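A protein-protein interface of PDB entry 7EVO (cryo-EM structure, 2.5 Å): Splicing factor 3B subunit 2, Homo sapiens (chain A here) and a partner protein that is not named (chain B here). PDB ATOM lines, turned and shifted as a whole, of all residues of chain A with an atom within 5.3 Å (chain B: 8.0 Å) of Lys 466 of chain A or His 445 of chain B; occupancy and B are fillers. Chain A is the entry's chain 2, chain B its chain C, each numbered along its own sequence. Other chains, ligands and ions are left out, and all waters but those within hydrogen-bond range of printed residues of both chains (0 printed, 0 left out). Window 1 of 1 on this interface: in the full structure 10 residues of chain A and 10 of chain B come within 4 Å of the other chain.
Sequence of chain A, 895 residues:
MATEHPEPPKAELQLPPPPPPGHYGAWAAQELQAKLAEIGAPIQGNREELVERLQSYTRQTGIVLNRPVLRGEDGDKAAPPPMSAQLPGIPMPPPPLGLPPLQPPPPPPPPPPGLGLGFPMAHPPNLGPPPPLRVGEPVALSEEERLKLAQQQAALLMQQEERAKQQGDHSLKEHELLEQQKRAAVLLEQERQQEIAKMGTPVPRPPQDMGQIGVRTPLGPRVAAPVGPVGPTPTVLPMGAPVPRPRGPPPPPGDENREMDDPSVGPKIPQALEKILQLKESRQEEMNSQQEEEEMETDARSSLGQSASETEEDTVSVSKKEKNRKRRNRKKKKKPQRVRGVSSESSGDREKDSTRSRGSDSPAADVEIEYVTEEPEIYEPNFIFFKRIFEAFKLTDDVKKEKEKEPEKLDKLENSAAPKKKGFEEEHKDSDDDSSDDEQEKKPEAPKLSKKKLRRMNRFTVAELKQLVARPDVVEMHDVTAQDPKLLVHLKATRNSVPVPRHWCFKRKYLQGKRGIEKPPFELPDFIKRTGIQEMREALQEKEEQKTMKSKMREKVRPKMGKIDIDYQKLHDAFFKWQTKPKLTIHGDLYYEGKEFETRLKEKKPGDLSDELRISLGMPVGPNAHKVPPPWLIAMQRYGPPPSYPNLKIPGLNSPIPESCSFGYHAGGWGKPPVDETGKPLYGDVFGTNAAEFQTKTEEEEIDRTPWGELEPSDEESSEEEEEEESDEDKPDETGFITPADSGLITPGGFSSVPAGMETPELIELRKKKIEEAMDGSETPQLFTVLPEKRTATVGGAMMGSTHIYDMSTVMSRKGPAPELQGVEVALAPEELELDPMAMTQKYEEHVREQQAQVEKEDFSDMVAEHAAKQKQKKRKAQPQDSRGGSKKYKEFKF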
ATOM      1  N   THR A 461      -4.869 -25.661 -31.123  1.00  0.00           N
ATOM      2  CA  THR A 461      -4.752 -24.292 -30.656  1.00  0.00           C
ATOM      3  C   THR A 461      -6.078 -23.856 -30.043  1.00  0.00           C
ATOM      4  O   THR A 461      -7.114 -24.500 -30.225  1.00  0.00           O
ATOM      5  CB  THR A 461      -4.355 -23.352 -31.796  1.00  0.00           C
ATOM      6  OG1 THR A 461      -5.479 -23.134 -32.658  1.00  0.00           O
ATOM      7  CG2 THR A 461      -3.206 -23.939 -32.602  1.00  0.00           C
ATOM      8  N   VAL A 462      -6.036 -22.752 -29.295  1.00  0.00           N
ATOM      9  CA  VAL A 462      -7.232 -22.295 -28.592  1.00  0.00           C
ATOM     10  C   VAL A 462      -8.353 -21.996 -29.578  1.00  0.00           C
ATOM     11  O   VAL A 462      -9.501 -22.413 -29.381  1.00  0.00           O
ATOM     12  CB  VAL A 462      -6.901 -21.072 -27.716  1.00  0.00           C
ATOM     13  CG1 VAL A 462      -8.174 -20.415 -27.223  1.00  0.00           C
ATOM     14  CG2 VAL A 462      -6.036 -21.488 -26.546  1.00  0.00           C
ATOM     15  N   ALA A 463      -8.036 -21.293 -30.667  1.00  0.00           N
ATOM     16  CA  ALA A 463      -9.064 -20.941 -31.640  1.00  0.00           C
ATOM     17  C   ALA A 463      -9.544 -22.166 -32.406  1.00  0.00           C
ATOM     18  O   ALA A 463     -10.714 -22.244 -32.798  1.00  0.00           O
ATOM     19  CB  ALA A 463      -8.534 -19.880 -32.602  1.00  0.00           C
ATOM     20  N   GLU A 464      -8.654 -23.133 -32.637  1.00  0.00           N
ATOM     21  CA  GLU A 464      -9.053 -24.348 -33.336  1.00  0.00           C
ATOM     22  C   GLU A 464      -9.984 -25.199 -32.481  1.00  0.00           C
ATOM     23  O   GLU A 464     -10.956 -25.770 -32.987  1.00  0.00           O
ATOM     24  CB  GLU A 464      -7.817 -25.148 -33.745  1.00  0.00           C
ATOM     25  CG  GLU A 464      -8.125 -26.512 -34.336  1.00  0.00           C
ATOM     26  CD  GLU A 464      -6.874 -27.262 -34.745  1.00  0.00           C
ATOM     27  OE1 GLU A 464      -5.764 -26.742 -34.507  1.00  0.00           O
ATOM     28  OE2 GLU A 464      -7.001 -28.370 -35.307  1.00  0.00           O
ATOM     29  N   LEU A 465      -9.703 -25.294 -31.179  1.00  0.00           N
ATOM     30  CA  LEU A 465     -10.567 -26.072 -30.297  1.00  0.00           C
ATOM     31  C   LEU A 465     -11.870 -25.334 -30.018  1.00  0.00           C
ATOM     32  O   LEU A 465     -12.909 -25.960 -29.775  1.00  0.00           O
ATOM     33  CB  LEU A 465      -9.828 -26.398 -28.997  1.00  0.00           C
ATOM     34  CG  LEU A 465     -10.629 -26.953 -27.817  1.00  0.00           C
ATOM     35  CD1 LEU A 465     -10.957 -28.421 -28.026  1.00  0.00           C
ATOM     36  CD2 LEU A 465      -9.864 -26.762 -26.519  1.00  0.00           C
ATOM     37  N   LYS A 466     -11.840 -23.999 -30.062  1.00  0.00           N
ATOM     38  CA  LYS A 466     -13.065 -23.227 -29.880  1.00  0.00           C
ATOM     39  C   LYS A 466     -14.037 -23.462 -31.030  1.00  0.00           C
ATOM     40  O   LYS A 466     -15.249 -23.271 -30.878  1.00  0.00           O
ATOM     41  CB  LYS A 466     -12.730 -21.742 -29.754  1.00  0.00           C
ATOM     42  CG  LYS A 466     -12.314 -21.304 -28.360  1.00  0.00           C
ATOM     43  CD  LYS A 466     -12.588 -19.827 -28.143  1.00  0.00           C
ATOM     44  CE  LYS A 466     -12.483 -19.454 -26.676  1.00  0.00           C
ATOM     45  NZ  LYS A 466     -11.087 -19.224 -26.236  1.00  0.00           N
ATOM     46  N   GLN A 467     -13.522 -23.879 -32.189  1.00  0.00           N
ATOM     47  CA  GLN A 467     -14.378 -24.120 -33.346  1.00  0.00           C
ATOM     48  C   GLN A 467     -15.050 -25.485 -33.269  1.00  0.00           C
ATOM     49  O   GLN A 467     -16.077 -25.717 -33.919  1.00  0.00           O
ATOM     50  CB  GLN A 467     -13.562 -24.007 -34.633  1.00  0.00           C
ATOM     51  CG  GLN A 467     -13.217 -22.587 -35.033  1.00  0.00           C
ATOM     52  CD  GLN A 467     -14.217 -22.004 -36.006  1.00  0.00           C
ATOM     53  OE1 GLN A 467     -14.826 -22.727 -36.793  1.00  0.00           O
ATOM     54  NE2 GLN A 467     -14.390 -20.691 -35.960  1.00  0.00           N
ATOM     55  N   LEU A 468     -14.477 -26.412 -32.501  1.00  0.00           N
ATOM     56  CA  LEU A 468     -15.011 -27.770 -32.465  1.00  0.00           C
ATOM     57  C   LEU A 468     -16.088 -27.925 -31.398  1.00  0.00           C
ATOM     58  O   LEU A 468     -17.020 -28.721 -31.559  1.00  0.00           O
ATOM     59  CB  LEU A 468     -13.879 -28.768 -32.233  1.00  0.00           C
ATOM     60  CG  LEU A 468     -12.894 -28.956 -33.389  1.00  0.00           C
ATOM     61  CD1 LEU A 468     -12.120 -30.252 -33.229  1.00  0.00           C
ATOM     62  CD2 LEU A 468     -13.623 -28.925 -34.723  1.00  0.00           C
ATOM     63  N   VAL A 469     -15.980 -27.175 -30.301  1.00  0.00           N
ATOM     64  CA  VAL A 469     -16.823 -27.423 -29.138  1.00  0.00           C
ATOM     65  C   VAL A 469     -18.141 -26.671 -29.266  1.00  0.00           C
ATOM     66  O   VAL A 469     -18.238 -25.652 -29.964  1.00  0.00           O
ATOM     67  CB  VAL A 469     -16.079 -27.031 -27.851  1.00  0.00           C
ATOM     68  CG1 VAL A 469     -14.779 -27.806 -27.750  1.00  0.00           C
ATOM     69  CG2 VAL A 469     -15.815 -25.536 -27.821  1.00  0.00           C
ATOM     70  N   PRO A 472     -17.821 -22.486 -26.588  1.00  0.00           N
ATOM     71  CA  PRO A 472     -16.420 -22.042 -26.632  1.00  0.00           C
ATOM     72  C   PRO A 472     -16.012 -21.151 -25.472  1.00  0.00           C
ATOM     73  O   PRO A 472     -14.809 -20.962 -25.258  1.00  0.00           O
ATOM     74  CB  PRO A 472     -16.336 -21.292 -27.968  1.00  0.00           C
ATOM     75  CG  PRO A 472     -17.722 -20.819 -28.216  1.00  0.00           C
ATOM     76  CD  PRO A 472     -18.647 -21.841 -27.622  1.00  0.00           C
ATOM     77  N   ASP A 473     -16.957 -20.603 -24.706  1.00  0.00           N
ATOM     78  CA  ASP A 473     -16.583 -19.627 -23.686  1.00  0.00           C
ATOM     79  C   ASP A 473     -16.067 -20.302 -22.419  1.00  0.00           C
ATOM     80  O   ASP A 473     -15.628 -19.624 -21.484  1.00  0.00           O
ATOM     81  CB  ASP A 473     -17.766 -18.716 -23.363  1.00  0.00           C
ATOM     82  CG  ASP A 473     -19.041 -19.485 -23.114  1.00  0.00           C
ATOM     83  OD1 ASP A 473     -19.103 -20.667 -23.503  1.00  0.00           O
ATOM     84  OD2 ASP A 473     -19.981 -18.910 -22.527  1.00  0.00           O
ATOM     85  N   VAL A 475     -13.665 -22.593 -22.739  1.00  0.00           N
ATOM     86  CA  VAL A 475     -12.298 -22.960 -23.087  1.00  0.00           C
ATOM     87  C   VAL A 475     -11.336 -21.917 -22.531  1.00  0.00           C
ATOM     88  O   VAL A 475     -11.615 -20.712 -22.548  1.00  0.00           O
ATOM     89  CB  VAL A 475     -12.160 -23.103 -24.612  1.00  0.00           C
ATOM     90  CG1 VAL A 475     -10.730 -23.440 -25.002  1.00  0.00           C
ATOM     91  CG2 VAL A 475     -13.113 -24.165 -25.128  1.00  0.00           C
ATOM     92  N   GLN B 423      -3.464 -12.305 -20.147  1.00  0.00           N
ATOM     93  CA  GLN B 423      -4.815 -12.845 -20.034  1.00  0.00           C
ATOM     94  C   GLN B 423      -5.816 -11.753 -19.681  1.00  0.00           C
ATOM     95  O   GLN B 423      -6.985 -11.818 -20.079  1.00  0.00           O
ATOM     96  CB  GLN B 423      -4.846 -13.961 -18.989  1.00  0.00           C
ATOM     97  CG  GLN B 423      -5.699 -15.161 -19.377  1.00  0.00           C
ATOM     98  CD  GLN B 423      -7.175 -14.822 -19.470  1.00  0.00           C
ATOM     99  OE1 GLN B 423      -7.777 -14.349 -18.506  1.00  0.00           O
ATOM    100  NE2 GLN B 423      -7.765 -15.063 -20.635  1.00  0.00           N
ATOM    101  N   MET B 435     -11.431  -4.877 -31.176  1.00  0.00           N
ATOM    102  CA  MET B 435     -12.522  -5.751 -31.590  1.00  0.00           C
ATOM    103  C   MET B 435     -13.672  -4.982 -32.220  1.00  0.00           C
ATOM    104  O   MET B 435     -14.330  -5.509 -33.123  1.00  0.00           O
ATOM    105  CB  MET B 435     -13.033  -6.566 -30.400  1.00  0.00           C
ATOM    106  CG  MET B 435     -12.164  -7.760 -30.049  1.00  0.00           C
ATOM    107  SD  MET B 435     -12.552  -9.220 -31.032  1.00  0.00           S
ATOM    108  CE  MET B 435     -14.071  -9.759 -30.252  1.00  0.00           C
ATOM    109  N   PRO B 441     -18.626  -8.078 -30.795  1.00  0.00           N
ATOM    110  CA  PRO B 441     -18.633  -7.667 -29.387  1.00  0.00           C
ATOM    111  C   PRO B 441     -17.596  -8.420 -28.570  1.00  0.00           C
ATOM    112  O   PRO B 441     -17.157  -9.513 -28.936  1.00  0.00           O
ATOM    113  CB  PRO B 441     -20.057  -8.003 -28.927  1.00  0.00           C
ATOM    114  CG  PRO B 441     -20.525  -9.052 -29.878  1.00  0.00           C
ATOM    115  CD  PRO B 441     -19.891  -8.719 -31.193  1.00  0.00           C
ATOM    116  N   ASN B 442     -17.205  -7.818 -27.450  1.00  0.00           N
ATOM    117  CA  ASN B 442     -16.270  -8.463 -26.537  1.00  0.00           C
ATOM    118  C   ASN B 442     -17.023  -9.302 -25.513  1.00  0.00           C
ATOM    119  O   ASN B 442     -17.694  -8.768 -24.626  1.00  0.00           O
ATOM    120  CB  ASN B 442     -15.413  -7.414 -25.831  1.00  0.00           C
ATOM    121  CG  ASN B 442     -13.951  -7.505 -26.212  1.00  0.00           C
ATOM    122  OD1 ASN B 442     -13.582  -8.228 -27.135  1.00  0.00           O
ATOM    123  ND2 ASN B 442     -13.108  -6.773 -25.496  1.00  0.00           N
ATOM    124  N   THR B 443     -16.907 -10.620 -25.636  1.00  0.00           N
ATOM    125  CA  THR B 443     -17.549 -11.532 -24.698  1.00  0.00           C
ATOM    126  C   THR B 443     -16.533 -12.583 -24.279  1.00  0.00           C
ATOM    127  O   THR B 443     -15.392 -12.596 -24.748  1.00  0.00           O
ATOM    128  CB  THR B 443     -18.796 -12.183 -25.307  1.00  0.00           C
ATOM    129  OG1 THR B 443     -18.574 -12.438 -26.699  1.00  0.00           O
ATOM    130  CG2 THR B 443     -20.006 -11.273 -25.150  1.00  0.00           C
ATOM    131  N   ALA B 444     -16.965 -13.469 -23.380  1.00  0.00           N
ATOM    132  CA  ALA B 444     -16.069 -14.509 -22.883  1.00  0.00           C
ATOM    133  C   ALA B 444     -15.733 -15.514 -23.976  1.00  0.00           C
ATOM    134  O   ALA B 444     -14.718 -16.215 -23.892  1.00  0.00           O
ATOM    135  CB  ALA B 444     -16.695 -15.210 -21.679  1.00  0.00           C
ATOM    136  N   HIS B 445     -16.575 -15.600 -25.010  1.00  0.00           N
ATOM    137  CA  HIS B 445     -16.289 -16.498 -26.123  1.00  0.00           C
ATOM    138  C   HIS B 445     -15.012 -16.092 -26.846  1.00  0.00           C
ATOM    139  O   HIS B 445     -14.228 -16.948 -27.266  1.00  0.00           O
ATOM    140  CB  HIS B 445     -17.461 -16.522 -27.103  1.00  0.00           C
ATOM    141  CG  HIS B 445     -18.793 -16.753 -26.458  1.00  0.00           C
ATOM    142  ND1 HIS B 445     -19.504 -17.921 -26.623  1.00  0.00           N
ATOM    143  CD2 HIS B 445     -19.549 -15.961 -25.663  1.00  0.00           C
ATOM    144  CE1 HIS B 445     -20.637 -17.843 -25.950  1.00  0.00           C
ATOM    145  NE2 HIS B 445     -20.690 -16.662 -25.358  1.00  0.00           N
ATOM    146  N   PHE B 446     -14.791 -14.788 -27.011  1.00  0.00           N
ATOM    147  CA  PHE B 446     -13.611 -14.290 -27.717  1.00  0.00           C
ATOM    148  C   PHE B 446     -12.527 -13.910 -26.709  1.00  0.00           C
ATOM    149  O   PHE B 446     -12.120 -12.755 -26.574  1.00  0.00           O
ATOM    150  CB  PHE B 446     -13.986 -13.122 -28.619  1.00  0.00           C
ATOM    151  CG  PHE B 446     -14.970 -13.484 -29.689  1.00  0.00           C
ATOM    152  CD1 PHE B 446     -14.549 -14.112 -30.848  1.00  0.00           C
ATOM    153  CD2 PHE B 446     -16.318 -13.211 -29.531  1.00  0.00           C
ATOM    154  CE1 PHE B 446     -15.452 -14.453 -31.834  1.00  0.00           C
ATOM    155  CE2 PHE B 446     -17.225 -13.550 -30.513  1.00  0.00           C
ATOM    156  CZ  PHE B 446     -16.792 -14.171 -31.665  1.00  0.00           C
ATOM    157  N   ALA B 447     -12.061 -14.925 -25.990  1.00  0.00           N
ATOM    158  CA  ALA B 447     -10.935 -14.793 -25.083  1.00  0.00           C
ATOM    159  C   ALA B 447      -9.843 -15.757 -25.520  1.00  0.00           C
ATOM    160  O   ALA B 447     -10.118 -16.836 -26.051  1.00  0.00           O
ATOM    161  CB  ALA B 447     -11.340 -15.064 -23.629  1.00  0.00           C
ATOM    162  N   ASN B 448      -8.593 -15.341 -25.306  1.00  0.00           N
ATOM    163  CA  ASN B 448      -7.415 -16.095 -25.740  1.00  0.00           C
ATOM    164  C   ASN B 448      -7.387 -16.284 -27.256  1.00  0.00           C
ATOM    165  O   ASN B 448      -6.666 -17.140 -27.772  1.00  0.00           O
ATOM    166  CB  ASN B 448      -7.319 -17.446 -25.026  1.00  0.00           C
ATOM    167  CG  ASN B 448      -7.430 -17.319 -23.522  1.00  0.00           C
ATOM    168  OD1 ASN B 448      -8.514 -17.446 -22.953  1.00  0.00           O
ATOM    169  ND2 ASN B 448      -6.305 -17.065 -22.866  1.00  0.00           N
ATOM    170  N   VAL B 449      -8.171 -15.488 -27.979  1.00  0.00           N
ATOM    171  CA  VAL B 449      -8.168 -15.472 -29.437  1.00  0.00           C
ATOM    172  C   VAL B 449      -7.501 -14.183 -29.889  1.00  0.00           C
ATOM    173  O   VAL B 449      -8.001 -13.086 -29.611  1.00  0.00           O
ATOM    174  CB  VAL B 449      -9.593 -15.588 -30.001  1.00  0.00           C
ATOM    175  CG1 VAL B 449      -9.598 -15.295 -31.493  1.00  0.00           C
ATOM    176  CG2 VAL B 449     -10.162 -16.967 -29.721  1.00  0.00           C
ATOM    177  N   ASP B 454      -9.470 -15.855 -37.303  1.00  0.00           N
ATOM    178  CA  ASP B 454     -10.046 -16.767 -36.322  1.00  0.00           C
ATOM    179  C   ASP B 454     -11.238 -16.125 -35.627  1.00  0.00           C
ATOM    180  O   ASP B 454     -12.274 -16.770 -35.427  1.00  0.00           O
ATOM    181  CB  ASP B 454      -8.988 -17.178 -35.299  1.00  0.00           C
ATOM    182  CG  ASP B 454      -8.028 -18.215 -35.840  1.00  0.00           C
ATOM    183  OD1 ASP B 454      -8.394 -18.926 -36.799  1.00  0.00           O
ATOM    184  OD2 ASP B 454      -6.905 -18.319 -35.305  1.00  0.00           O
ATOM    185  N   LEU B 458     -15.059 -17.526 -35.861  1.00  0.00           N
ATOM    186  CA  LEU B 458     -15.789 -17.910 -34.659  1.00  0.00           C
ATOM    187  C   LEU B 458     -17.033 -17.049 -34.482  1.00  0.00           C
ATOM    188  O   LEU B 458     -18.048 -17.512 -33.949  1.00  0.00           O
ATOM    189  CB  LEU B 458     -14.876 -17.809 -33.437  1.00  0.00           C
ATOM    190  CG  LEU B 458     -15.397 -18.443 -32.147  1.00  0.00           C
ATOM    191  CD1 LEU B 458     -15.197 -19.950 -32.185  1.00  0.00           C
ATOM    192  CD2 LEU B 458     -14.705 -17.841 -30.938  1.00  0.00           C
ATOM    193  N   TRP B 459     -16.987 -15.803 -34.959  1.00  0.00           N
ATOM    194  CA  TRP B 459     -18.176 -14.961 -34.921  1.00  0.00           C
ATOM    195  C   TRP B 459     -19.240 -15.470 -35.880  1.00  0.00           C
ATOM    196  O   TRP B 459     -20.429 -15.485 -35.545  1.00  0.00           O
ATOM    197  CB  TRP B 459     -17.807 -13.514 -35.244  1.00  0.00           C
ATOM    198  CG  TRP B 459     -18.988 -12.599 -35.289  1.00  0.00           C
ATOM    199  CD1 TRP B 459     -19.420 -11.872 -36.359  1.00  0.00           C
ATOM    200  CD2 TRP B 459     -19.898 -12.314 -34.219  1.00  0.00           C
ATOM    201  NE1 TRP B 459     -20.537 -11.150 -36.022  1.00  0.00           N
ATOM    202  CE2 TRP B 459     -20.852 -11.404 -34.714  1.00  0.00           C
ATOM    203  CE3 TRP B 459     -19.996 -12.738 -32.891  1.00  0.00           C
ATOM    204  CZ2 TRP B 459     -21.891 -10.913 -33.928  1.00  0.00           C
ATOM    205  CZ3 TRP B 459     -21.029 -12.248 -32.113  1.00  0.00           C
ATOM    206  CH2 TRP B 459     -21.961 -11.345 -32.633  1.00  0.00           C
ATOM    207  N   LYS B 461     -19.593 -18.577 -36.720  1.00  0.00           N
ATOM    208  CA  LYS B 461     -20.110 -19.782 -36.077  1.00  0.00           C
ATOM    209  C   LYS B 461     -21.122 -19.448 -34.985  1.00  0.00           C
ATOM    210  O   LYS B 461     -22.212 -20.036 -34.934  1.00  0.00           O
ATOM    211  CB  LYS B 461     -18.960 -20.598 -35.493  1.00  0.00           C
ATOM    212  CG  LYS B 461     -19.400 -21.887 -34.829  1.00  0.00           C
ATOM    213  CD  LYS B 461     -18.271 -22.895 -34.780  1.00  0.00           C
ATOM    214  CE  LYS B 461     -17.950 -23.263 -33.340  1.00  0.00           C
ATOM    215  NZ  LYS B 461     -18.847 -24.329 -32.813  1.00  0.00           N
ATOM    216  N   LEU B 462     -20.768 -18.524 -34.089  1.00  0.00           N
ATOM    217  CA  LEU B 462     -21.662 -18.170 -32.992  1.00  0.00           C
ATOM    218  C   LEU B 462     -22.944 -17.531 -33.508  1.00  0.00           C
ATOM    219  O   LEU B 462     -24.032 -17.785 -32.975  1.00  0.00           O
ATOM    220  CB  LEU B 462     -20.950 -17.231 -32.021  1.00  0.00           C
ATOM    221  CG  LEU B 462     -20.053 -17.898 -30.979  1.00  0.00           C
ATOM    222  CD1 LEU B 462     -19.291 -16.849 -30.193  1.00  0.00           C
ATOM    223  CD2 LEU B 462     -20.867 -18.786 -30.048  1.00  0.00           C
ATOM    224  N   GLN B 465     -25.136 -20.358 -34.861  1.00  0.00           N
ATOM    225  CA  GLN B 465     -25.696 -21.102 -33.734  1.00  0.00           C
ATOM    226  C   GLN B 465     -26.845 -20.357 -33.062  1.00  0.00           C
ATOM    227  O   GLN B 465     -27.959 -20.893 -32.954  1.00  0.00           O
ATOM    228  CB  GLN B 465     -24.601 -21.381 -32.706  1.00  0.00           C
ATOM    229  CG  GLN B 465     -24.902 -22.520 -31.752  1.00  0.00           C
ATOM    230  CD  GLN B 465     -24.000 -22.504 -30.536  1.00  0.00           C
ATOM    231  OE1 GLN B 465     -24.468 -22.393 -29.404  1.00  0.00           O
ATOM    232  NE2 GLN B 465     -22.696 -22.611 -30.763  1.00  0.00           N
ATOM    233  N   LYS B 466     -26.598 -19.126 -32.607  1.00  0.00           N
ATOM    234  CA  LYS B 466     -27.627 -18.395 -31.880  1.00  0.00           C
ATOM    235  C   LYS B 466     -28.832 -18.108 -32.765  1.00  0.00           C
ATOM    236  O   LYS B 466     -29.972 -18.367 -32.365  1.00  0.00           O
ATOM    237  CB  LYS B 466     -27.053 -17.104 -31.296  1.00  0.00           C
ATOM    238  CG  LYS B 466     -26.740 -17.212 -29.811  1.00  0.00           C
ATOM    239  CD  LYS B 466     -26.040 -15.973 -29.274  1.00  0.00           C
ATOM    240  CE  LYS B 466     -24.751 -15.678 -30.025  1.00  0.00           C
ATOM    241  NZ  LYS B 466     -24.304 -14.271 -29.809  1.00  0.00           N
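The side-chain amide nitrogen (NE2) of Gln 423 of chain B sits close to the side-chain amide nitrogen (ND2) of Asn 448 of chain B (3.3 Å).
Of chain B, only His 445 (3.1 Å), Ala 447 (2.6 Å), Leu 458 (3.6 Å) and Lys 461 (3.7 Å) come within 4 Å of Lys 466 of chain A. Of the printed residues of chain B, Gln 467 of chain A touches Leu 458 (3.2 Å) and Lys 461 (3.1 Å). Of the printed residues of chain B, Val 469 of chain A touches Lys 461 (3.2 Å). Of the printed residues of chain B, Pro 472 of chain A touches His 445. Met 435 of chain B touches none of the printed residues of chain A. His 445 of chain B touches just these residues of chain A: Lys 466 (3.1 Å), Pro 472 (3.8 Å) and Asp 473 (3.6 Å). Of the printed residues of chain A, Asp 454 of chain B touches Ala 463 (3.5 Å). Of the printed residues of chain A, Lys 461 of chain B touches Lys 466 (3.7 Å), Gln 467 (3.1 Å) and Val 469 (3.2 Å). The nearest residue of chain B that does not touch Lys 466 of chain A is Val 449 of chain B (4.1 Å). The nearest printed residue of chain A that does not touch His 445 of chain B is Val 475 of chain A (6.6 Å). The nearest printed residue of chain B that does not touch Ala 463 of chain A is Val 449 of chain B (4.4 Å).
Among the printed residues, pairs that only touch across the chains: Lys 466 of chain A with His 445 of chain B, Ala 463 of chain A with Asp 454 of chain B, Lys 466 of chain A with Leu 458 of chain B, Asp 473 of chain A with His 445 of chain B, Val 462 of chain A with Asn 448 of chain B, Lys 466 of chain A with Lys 461 of chain B, Pro 472 of chain A with His 445 of chain B and Asp 473 of chain A with Ala 444 of chain B.
Hydrophobic or aromatic side chains of chain A that line the printed part of chain B: Val 462, Ala 463 and Pro 472. Along chain B the printed residues that touch a printed residue of chain A span positions 444 to 461. Among the printed residues, no Asp or Glu carboxylate lies within 4 Å of a Lys or Arg side-chain nitrogen of the other chain.
The backbone carbonyl oxygen (O) of Gln 467 of chain A sits close to the side-chain amino group (NZ) of Lys 461 of chain B, 3.3 Å away. The backbone carbonyl oxygen (O) of Ala 447 of chain B sits at hydrogen-bond distance from the side-chain amino group (NZ) of Lys 466 of chain A, 2.6 Å away. The backbone NH (N) of Leu 458 of chain B sits close to the side-chain amide nitrogen (NE2) of Gln 467 of chain A (3.2 Å). The side-chain amino group (NZ) of Lys 461 of chain B sits at hydrogen-bond distance from the backbone carbonyl oxygen (O) of Val 469 of chain A (3.2 Å).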
